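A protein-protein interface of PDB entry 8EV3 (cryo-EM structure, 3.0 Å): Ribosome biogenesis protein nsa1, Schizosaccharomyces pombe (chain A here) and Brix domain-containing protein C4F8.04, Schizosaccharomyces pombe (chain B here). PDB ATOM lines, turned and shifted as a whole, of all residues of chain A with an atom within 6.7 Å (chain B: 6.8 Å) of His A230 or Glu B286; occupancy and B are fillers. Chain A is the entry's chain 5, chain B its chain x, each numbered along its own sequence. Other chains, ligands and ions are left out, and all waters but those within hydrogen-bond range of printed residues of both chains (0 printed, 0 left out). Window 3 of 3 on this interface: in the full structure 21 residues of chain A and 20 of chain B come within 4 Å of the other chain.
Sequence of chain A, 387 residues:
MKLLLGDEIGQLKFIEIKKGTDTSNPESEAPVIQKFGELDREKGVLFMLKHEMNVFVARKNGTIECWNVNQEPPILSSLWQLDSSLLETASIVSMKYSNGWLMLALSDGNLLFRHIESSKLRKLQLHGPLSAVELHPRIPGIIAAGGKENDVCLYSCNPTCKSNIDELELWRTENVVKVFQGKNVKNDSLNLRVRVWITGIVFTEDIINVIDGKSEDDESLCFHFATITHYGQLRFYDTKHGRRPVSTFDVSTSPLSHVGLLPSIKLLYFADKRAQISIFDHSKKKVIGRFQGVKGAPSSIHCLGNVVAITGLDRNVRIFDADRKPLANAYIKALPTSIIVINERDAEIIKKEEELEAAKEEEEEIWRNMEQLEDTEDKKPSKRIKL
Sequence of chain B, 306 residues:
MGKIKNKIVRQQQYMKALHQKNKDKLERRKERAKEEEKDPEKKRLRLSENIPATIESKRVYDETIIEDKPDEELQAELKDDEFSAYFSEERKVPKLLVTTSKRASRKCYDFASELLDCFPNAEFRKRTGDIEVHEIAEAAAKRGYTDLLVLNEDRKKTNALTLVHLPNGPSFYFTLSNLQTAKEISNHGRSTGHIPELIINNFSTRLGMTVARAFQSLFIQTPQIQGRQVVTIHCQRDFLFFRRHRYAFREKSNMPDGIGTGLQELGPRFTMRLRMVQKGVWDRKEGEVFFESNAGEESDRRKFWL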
ATOM      1  N   ARG A 195      24.688 -18.176 -13.649  1.00  0.00           N
ATOM      2  CA  ARG A 195      25.181 -17.508 -12.456  1.00  0.00           C
ATOM      3  C   ARG A 195      25.471 -18.519 -11.354  1.00  0.00           C
ATOM      4  O   ARG A 195      24.829 -19.566 -11.256  1.00  0.00           O
ATOM      5  CB  ARG A 195      24.174 -16.467 -11.979  1.00  0.00           C
ATOM      6  CG  ARG A 195      24.046 -15.288 -12.918  1.00  0.00           C
ATOM      7  CD  ARG A 195      22.848 -14.440 -12.577  1.00  0.00           C
ATOM      8  NE  ARG A 195      21.595 -15.145 -12.813  1.00  0.00           N
ATOM      9  CZ  ARG A 195      20.398 -14.629 -12.579  1.00  0.00           C
ATOM     10  NH1 ARG A 195      20.254 -13.397 -12.120  1.00  0.00           N
ATOM     11  NH2 ARG A 195      19.316 -15.367 -12.807  1.00  0.00           N
ATOM     12  N   VAL A 196      26.456 -18.196 -10.524  1.00  0.00           N
ATOM     13  CA  VAL A 196      26.935 -19.095  -9.481  1.00  0.00           C
ATOM     14  C   VAL A 196      26.638 -18.466  -8.129  1.00  0.00           C
ATOM     15  O   VAL A 196      27.046 -17.331  -7.858  1.00  0.00           O
ATOM     16  CB  VAL A 196      28.435 -19.392  -9.637  1.00  0.00           C
ATOM     17  CG1 VAL A 196      29.161 -18.179 -10.180  1.00  0.00           C
ATOM     18  CG2 VAL A 196      29.030 -19.825  -8.312  1.00  0.00           C
ATOM     19  N   TRP A 197      25.908 -19.198  -7.289  1.00  0.00           N
ATOM     20  CA  TRP A 197      25.661 -18.786  -5.910  1.00  0.00           C
ATOM     21  C   TRP A 197      25.453 -20.067  -5.108  1.00  0.00           C
ATOM     22  O   TRP A 197      24.342 -20.597  -5.067  1.00  0.00           O
ATOM     23  CB  TRP A 197      24.457 -17.857  -5.818  1.00  0.00           C
ATOM     24  CG  TRP A 197      24.184 -17.295  -4.446  1.00  0.00           C
ATOM     25  CD1 TRP A 197      24.624 -17.783  -3.252  1.00  0.00           C
ATOM     26  CD2 TRP A 197      23.399 -16.136  -4.135  1.00  0.00           C
ATOM     27  NE1 TRP A 197      24.166 -17.004  -2.221  1.00  0.00           N
ATOM     28  CE2 TRP A 197      23.411 -15.986  -2.737  1.00  0.00           C
ATOM     29  CE3 TRP A 197      22.687 -15.214  -4.906  1.00  0.00           C
ATOM     30  CZ2 TRP A 197      22.741 -14.949  -2.093  1.00  0.00           C
ATOM     31  CZ3 TRP A 197      22.020 -14.186  -4.263  1.00  0.00           C
ATOM     32  CH2 TRP A 197      22.054 -14.063  -2.872  1.00  0.00           C
ATOM     33  N   ILE A 198      26.520 -20.548  -4.470  1.00  0.00           N
ATOM     34  CA  ILE A 198      26.425 -21.758  -3.666  1.00  0.00           C
ATOM     35  C   ILE A 198      25.701 -21.445  -2.366  1.00  0.00           C
ATOM     36  O   ILE A 198      25.962 -20.425  -1.716  1.00  0.00           O
ATOM     37  CB  ILE A 198      27.822 -22.338  -3.398  1.00  0.00           C
ATOM     38  CG1 ILE A 198      28.600 -22.476  -4.704  1.00  0.00           C
ATOM     39  CG2 ILE A 198      27.718 -23.680  -2.701  1.00  0.00           C
ATOM     40  CD1 ILE A 198      28.189 -23.664  -5.534  1.00  0.00           C
ATOM     41  N   THR A 199      24.776 -22.316  -1.985  1.00  0.00           N
ATOM     42  CA  THR A 199      23.985 -22.119  -0.780  1.00  0.00           C
ATOM     43  C   THR A 199      24.106 -23.264   0.216  1.00  0.00           C
ATOM     44  O   THR A 199      24.020 -23.026   1.422  1.00  0.00           O
ATOM     45  CB  THR A 199      22.508 -21.908  -1.154  1.00  0.00           C
ATOM     46  OG1 THR A 199      22.363 -20.636  -1.792  1.00  0.00           O
ATOM     47  CG2 THR A 199      21.636 -21.908   0.075  1.00  0.00           C
ATOM     48  N   ILE A 228      23.825 -27.102  -3.574  1.00  0.00           N
ATOM     49  CA  ILE A 228      22.563 -26.481  -3.949  1.00  0.00           C
ATOM     50  C   ILE A 228      22.802 -24.989  -4.113  1.00  0.00           C
ATOM     51  O   ILE A 228      23.592 -24.394  -3.374  1.00  0.00           O
ATOM     52  CB  ILE A 228      21.446 -26.753  -2.922  1.00  0.00           C
ATOM     53  CG1 ILE A 228      21.879 -26.327  -1.523  1.00  0.00           C
ATOM     54  CG2 ILE A 228      21.062 -28.217  -2.940  1.00  0.00           C
ATOM     55  CD1 ILE A 228      20.743 -25.885  -0.646  1.00  0.00           C
ATOM     56  N   THR A 229      22.134 -24.392  -5.091  1.00  0.00           N
ATOM     57  CA  THR A 229      22.393 -23.016  -5.480  1.00  0.00           C
ATOM     58  C   THR A 229      21.170 -22.141  -5.247  1.00  0.00           C
ATOM     59  O   THR A 229      20.049 -22.625  -5.076  1.00  0.00           O
ATOM     60  CB  THR A 229      22.814 -22.936  -6.950  1.00  0.00           C
ATOM     61  OG1 THR A 229      21.712 -23.309  -7.782  1.00  0.00           O
ATOM     62  CG2 THR A 229      23.981 -23.869  -7.220  1.00  0.00           C
ATOM     63  N   HIS A 230      21.409 -20.829  -5.249  1.00  0.00           N
ATOM     64  CA  HIS A 230      20.350 -19.842  -5.093  1.00  0.00           C
ATOM     65  C   HIS A 230      19.383 -19.828  -6.268  1.00  0.00           C
ATOM     66  O   HIS A 230      18.308 -19.233  -6.160  1.00  0.00           O
ATOM     67  CB  HIS A 230      20.976 -18.459  -4.899  1.00  0.00           C
ATOM     68  CG  HIS A 230      20.002 -17.326  -4.981  1.00  0.00           C
ATOM     69  ND1 HIS A 230      19.192 -16.963  -3.928  1.00  0.00           N
ATOM     70  CD2 HIS A 230      19.711 -16.473  -5.990  1.00  0.00           C
ATOM     71  CE1 HIS A 230      18.442 -15.936  -4.286  1.00  0.00           C
ATOM     72  NE2 HIS A 230      18.739 -15.618  -5.532  1.00  0.00           N
ATOM     73  N   TYR A 231      19.723 -20.471  -7.380  1.00  0.00           N
ATOM     74  CA  TYR A 231      18.858 -20.498  -8.549  1.00  0.00           C
ATOM     75  C   TYR A 231      18.150 -21.835  -8.710  1.00  0.00           C
ATOM     76  O   TYR A 231      17.743 -22.187  -9.821  1.00  0.00           O
ATOM     77  CB  TYR A 231      19.669 -20.139  -9.793  1.00  0.00           C
ATOM     78  CG  TYR A 231      20.456 -18.865  -9.598  1.00  0.00           C
ATOM     79  CD1 TYR A 231      19.870 -17.629  -9.808  1.00  0.00           C
ATOM     80  CD2 TYR A 231      21.772 -18.897  -9.169  1.00  0.00           C
ATOM     81  CE1 TYR A 231      20.575 -16.464  -9.616  1.00  0.00           C
ATOM     82  CE2 TYR A 231      22.484 -17.736  -8.974  1.00  0.00           C
ATOM     83  CZ  TYR A 231      21.882 -16.523  -9.200  1.00  0.00           C
ATOM     84  OH  TYR A 231      22.588 -15.361  -9.006  1.00  0.00           O
ATOM     85  N   GLY A 232      17.986 -22.575  -7.620  1.00  0.00           N
ATOM     86  CA  GLY A 232      17.256 -23.829  -7.629  1.00  0.00           C
ATOM     87  C   GLY A 232      17.904 -24.942  -8.417  1.00  0.00           C
ATOM     88  O   GLY A 232      17.203 -25.710  -9.086  1.00  0.00           O
ATOM     89  N   GLN A 233      19.226 -25.059  -8.354  1.00  0.00           N
ATOM     90  CA  GLN A 233      19.955 -26.085  -9.084  1.00  0.00           C
ATOM     91  C   GLN A 233      20.700 -26.977  -8.106  1.00  0.00           C
ATOM     92  O   GLN A 233      21.482 -26.488  -7.285  1.00  0.00           O
ATOM     93  CB  GLN A 233      20.929 -25.460 -10.084  1.00  0.00           C
ATOM     94  CG  GLN A 233      20.377 -24.246 -10.803  1.00  0.00           C
ATOM     95  CD  GLN A 233      21.302 -23.736 -11.883  1.00  0.00           C
ATOM     96  OE1 GLN A 233      22.056 -24.502 -12.479  1.00  0.00           O
ATOM     97  NE2 GLN A 233      21.248 -22.437 -12.145  1.00  0.00           N
ATOM     98  N   THR A 253      12.258 -23.547  -8.595  1.00  0.00           N
ATOM     99  CA  THR A 253      12.411 -22.191  -9.104  1.00  0.00           C
ATOM    100  C   THR A 253      12.918 -21.239  -8.032  1.00  0.00           C
ATOM    101  O   THR A 253      13.700 -20.331  -8.327  1.00  0.00           O
ATOM    102  CB  THR A 253      11.082 -21.679  -9.661  1.00  0.00           C
ATOM    103  OG1 THR A 253      10.115 -21.612  -8.608  1.00  0.00           O
ATOM    104  CG2 THR A 253      10.570 -22.606 -10.742  1.00  0.00           C
ATOM    105  N   SER A 254      12.482 -21.433  -6.795  1.00  0.00           N
ATOM    106  CA  SER A 254      12.926 -20.628  -5.672  1.00  0.00           C
ATOM    107  C   SER A 254      14.302 -21.093  -5.200  1.00  0.00           C
ATOM    108  O   SER A 254      14.674 -22.251  -5.402  1.00  0.00           O
ATOM    109  CB  SER A 254      11.922 -20.724  -4.529  1.00  0.00           C
ATOM    110  OG  SER A 254      12.083 -19.661  -3.608  1.00  0.00           O
ATOM    111  N   PRO A 255      15.081 -20.204  -4.585  1.00  0.00           N
ATOM    112  CA  PRO A 255      16.394 -20.607  -4.071  1.00  0.00           C
ATOM    113  C   PRO A 255      16.288 -21.760  -3.088  1.00  0.00           C
ATOM    114  O   PRO A 255      15.360 -21.834  -2.284  1.00  0.00           O
ATOM    115  CB  PRO A 255      16.918 -19.338  -3.388  1.00  0.00           C
ATOM    116  CG  PRO A 255      15.826 -18.325  -3.487  1.00  0.00           C
ATOM    117  CD  PRO A 255      14.923 -18.746  -4.583  1.00  0.00           C
ATOM    118  N   LEU A 256      17.246 -22.671  -3.172  1.00  0.00           N
ATOM    119  CA  LEU A 256      17.300 -23.788  -2.250  1.00  0.00           C
ATOM    120  C   LEU A 256      17.928 -23.344  -0.937  1.00  0.00           C
ATOM    121  O   LEU A 256      18.819 -22.494  -0.910  1.00  0.00           O
ATOM    122  CB  LEU A 256      18.086 -24.945  -2.862  1.00  0.00           C
ATOM    123  CG  LEU A 256      17.442 -25.555  -4.105  1.00  0.00           C
ATOM    124  CD1 LEU A 256      18.399 -26.490  -4.793  1.00  0.00           C
ATOM    125  CD2 LEU A 256      16.170 -26.284  -3.744  1.00  0.00           C
ATOM    126  N   LYS A 273      13.004 -22.090  -0.402  1.00  0.00           N
ATOM    127  CA  LYS A 273      12.354 -21.028   0.352  1.00  0.00           C
ATOM    128  C   LYS A 273      10.853 -20.952   0.108  1.00  0.00           C
ATOM    129  O   LYS A 273      10.175 -20.163   0.770  1.00  0.00           O
ATOM    130  CB  LYS A 273      13.017 -19.692   0.024  1.00  0.00           C
ATOM    131  CG  LYS A 273      14.530 -19.790  -0.045  1.00  0.00           C
ATOM    132  CD  LYS A 273      15.219 -18.601   0.593  1.00  0.00           C
ATOM    133  CE  LYS A 273      14.962 -17.333  -0.188  1.00  0.00           C
ATOM    134  NZ  LYS A 273      16.123 -16.408  -0.126  1.00  0.00           N
ATOM    135  N   ARG A 274      10.318 -21.751  -0.813  1.00  0.00           N
ATOM    136  CA  ARG A 274       8.884 -21.831  -1.044  1.00  0.00           C
ATOM    137  C   ARG A 274       8.209 -22.877  -0.168  1.00  0.00           C
ATOM    138  O   ARG A 274       7.069 -23.263  -0.449  1.00  0.00           O
ATOM    139  CB  ARG A 274       8.602 -22.126  -2.518  1.00  0.00           C
ATOM    140  CG  ARG A 274       8.471 -20.889  -3.389  1.00  0.00           C
ATOM    141  CD  ARG A 274       7.232 -20.085  -3.035  1.00  0.00           C
ATOM    142  NE  ARG A 274       7.278 -18.738  -3.593  1.00  0.00           N
ATOM    143  CZ  ARG A 274       6.435 -18.274  -4.505  1.00  0.00           C
ATOM    144  NH1 ARG A 274       5.452 -19.020  -4.981  1.00  0.00           N
ATOM    145  NH2 ARG A 274       6.582 -17.031  -4.950  1.00  0.00           N
ATOM    146  N   GLN B 278       5.609 -12.549   2.812  1.00  0.00           N
ATOM    147  CA  GLN B 278       7.014 -12.827   2.571  1.00  0.00           C
ATOM    148  C   GLN B 278       7.860 -12.174   3.650  1.00  0.00           C
ATOM    149  O   GLN B 278       7.617 -11.026   4.032  1.00  0.00           O
ATOM    150  CB  GLN B 278       7.454 -12.319   1.198  1.00  0.00           C
ATOM    151  CG  GLN B 278       6.931 -13.129   0.037  1.00  0.00           C
ATOM    152  CD  GLN B 278       7.847 -13.061  -1.159  1.00  0.00           C
ATOM    153  OE1 GLN B 278       8.488 -12.042  -1.402  1.00  0.00           O
ATOM    154  NE2 GLN B 278       7.912 -14.144  -1.920  1.00  0.00           N
ATOM    155  N   VAL B 281      11.832  -8.016   1.693  1.00  0.00           N
ATOM    156  CA  VAL B 281      11.259  -7.264   0.588  1.00  0.00           C
ATOM    157  C   VAL B 281      10.629  -8.221  -0.420  1.00  0.00           C
ATOM    158  O   VAL B 281      11.021  -9.389  -0.536  1.00  0.00           O
ATOM    159  CB  VAL B 281      12.330  -6.381  -0.073  1.00  0.00           C
ATOM    160  CG1 VAL B 281      11.687  -5.345  -0.971  1.00  0.00           C
ATOM    161  CG2 VAL B 281      13.169  -5.702   0.988  1.00  0.00           C
ATOM    162  N   ASP B 283       9.848 -10.293  -3.374  1.00  0.00           N
ATOM    163  CA  ASP B 283      10.412 -10.893  -4.577  1.00  0.00           C
ATOM    164  C   ASP B 283       9.613 -12.158  -4.850  1.00  0.00           C
ATOM    165  O   ASP B 283       9.765 -13.152  -4.134  1.00  0.00           O
ATOM    166  CB  ASP B 283      11.897 -11.205  -4.403  1.00  0.00           C
ATOM    167  CG  ASP B 283      12.578 -11.540  -5.711  1.00  0.00           C
ATOM    168  OD1 ASP B 283      11.927 -11.422  -6.769  1.00  0.00           O
ATOM    169  OD2 ASP B 283      13.767 -11.918  -5.684  1.00  0.00           O
ATOM    170  N   ARG B 284       8.755 -12.117  -5.871  1.00  0.00           N
ATOM    171  CA  ARG B 284       7.807 -13.207  -6.073  1.00  0.00           C
ATOM    172  C   ARG B 284       8.524 -14.503  -6.427  1.00  0.00           C
ATOM    173  O   ARG B 284       8.059 -15.596  -6.086  1.00  0.00           O
ATOM    174  CB  ARG B 284       6.783 -12.832  -7.146  1.00  0.00           C
ATOM    175  CG  ARG B 284       7.161 -13.212  -8.564  1.00  0.00           C
ATOM    176  CD  ARG B 284       5.948 -13.220  -9.474  1.00  0.00           C
ATOM    177  NE  ARG B 284       4.979 -14.224  -9.053  1.00  0.00           N
ATOM    178  CZ  ARG B 284       5.002 -15.495  -9.429  1.00  0.00           C
ATOM    179  NH1 ARG B 284       5.935 -15.956 -10.243  1.00  0.00           N
ATOM    180  NH2 ARG B 284       4.070 -16.325  -8.970  1.00  0.00           N
ATOM    181  N   LYS B 285       9.662 -14.404  -7.113  1.00  0.00           N
ATOM    182  CA  LYS B 285      10.410 -15.608  -7.457  1.00  0.00           C
ATOM    183  C   LYS B 285      11.219 -16.121  -6.273  1.00  0.00           C
ATOM    184  O   LYS B 285      11.164 -17.312  -5.949  1.00  0.00           O
ATOM    185  CB  LYS B 285      11.330 -15.341  -8.648  1.00  0.00           C
ATOM    186  CG  LYS B 285      10.638 -14.897  -9.925  1.00  0.00           C
ATOM    187  CD  LYS B 285       9.490 -15.825 -10.294  1.00  0.00           C
ATOM    188  CE  LYS B 285       8.855 -15.425 -11.623  1.00  0.00           C
ATOM    189  NZ  LYS B 285       8.157 -14.115 -11.574  1.00  0.00           N
ATOM    190  N   GLU B 286      11.968 -15.239  -5.614  1.00  0.00           N
ATOM    191  CA  GLU B 286      12.998 -15.670  -4.677  1.00  0.00           C
ATOM    192  C   GLU B 286      12.793 -15.107  -3.278  1.00  0.00           C
ATOM    193  O   GLU B 286      13.747 -14.641  -2.651  1.00  0.00           O
ATOM    194  CB  GLU B 286      14.375 -15.264  -5.204  1.00  0.00           C
ATOM    195  CG  GLU B 286      14.468 -15.214  -6.719  1.00  0.00           C
ATOM    196  CD  GLU B 286      15.645 -14.395  -7.205  1.00  0.00           C
ATOM    197  OE1 GLU B 286      16.485 -14.002  -6.370  1.00  0.00           O
ATOM    198  OE2 GLU B 286      15.731 -14.140  -8.424  1.00  0.00           O
ATOM    199  N   GLY B 287      11.564 -15.153  -2.776  1.00  0.00           N
ATOM    200  CA  GLY B 287      11.244 -14.651  -1.454  1.00  0.00           C
ATOM    201  C   GLY B 287      11.027 -15.781  -0.468  1.00  0.00           C
ATOM    202  O   GLY B 287      10.635 -16.885  -0.847  1.00  0.00           O
ATOM    203  N   GLU B 288      11.286 -15.496   0.807  1.00  0.00           N
ATOM    204  CA  GLU B 288      11.049 -16.452   1.883  1.00  0.00           C
ATOM    205  C   GLU B 288       9.571 -16.412   2.241  1.00  0.00           C
ATOM    206  O   GLU B 288       9.075 -15.397   2.739  1.00  0.00           O
ATOM    207  CB  GLU B 288      11.910 -16.116   3.095  1.00  0.00           C
ATOM    208  CG  GLU B 288      13.394 -16.345   2.895  1.00  0.00           C
ATOM    209  CD  GLU B 288      13.941 -17.443   3.782  1.00  0.00           C
ATOM    210  OE1 GLU B 288      13.138 -18.252   4.288  1.00  0.00           O
ATOM    211  OE2 GLU B 288      15.174 -17.493   3.976  1.00  0.00           O
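The guanidinium group (NH2) of Arg A274 sits close to the backbone carbonyl oxygen (O) of Arg B284, at 2.4 Å.
The backbone carbonyl oxygen (O) of Lys B285 is in hydrogen-bond range of the side-chain hydroxyl (OG) of Ser A254 (3.4 Å).
The side-chain carboxylate (OE1) of Glu B286 lies within hydrogen-bond range of a ring nitrogen (NE2) of His A230, 2.9 Å away.
The backbone NH (N) of Lys A273 sits at hydrogen-bond distance from the backbone carbonyl oxygen (O) of Pro A255, at 3.0 Å.
The backbone NH (N) of His A230 is in hydrogen-bond range of the backbone carbonyl oxygen (O) of Trp A197, at 2.9 Å.
Among the printed residues, pairs that only touch across the chains: Pro A255 with Glu B286 (3.6 Å), Lys A273 with Glu B286 (3.8 Å), Lys A273 with Gly B287 (3.7 Å) and Lys A273 with Glu B288 (3.6 Å).
Of chain B, only Glu B286 comes within 4 Å of His A230.
Of chain A, only His A230, Pro A255 and Lys A273 come within 4 Å of Glu B286.
Of the printed residues of chain B, Pro A255 touches Glu B286 (3.6 Å).
Printed residues of chain A within 4 Å of Glu B288: Lys A273 (3.6 Å).
Of the printed residues of chain A, Arg B284 touches Arg A274 (2.4 Å).
Printed residues of chain A within 4 Å of Gly B287: Lys A273 (3.7 Å).
Printed residues of chain B within 4 Å of Arg A274: Arg B284.
Ile A198 touches none of the printed residues of chain B.
Thr A229 touches none of the printed residues of chain B.
The nearest residue of chain B that does not touch His A230 is Asp B283 (6.2 Å).
The nearest printed residue of chain A that does not touch Lys B285 is Pro A255 (4.2 Å).
Printed residues of chain B that touch a printed residue of chain A: Arg B284, Lys B285, Glu B286, Gly B287 and Glu B288.
Hydrophobic or aromatic side chains of chain A that line the printed part of chain B: His A230 and Pro A255.
Among the printed residues, no Asp or Glu carboxylate lies within 4 Å of a Lys or Arg side-chain nitrogen of the other chain.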
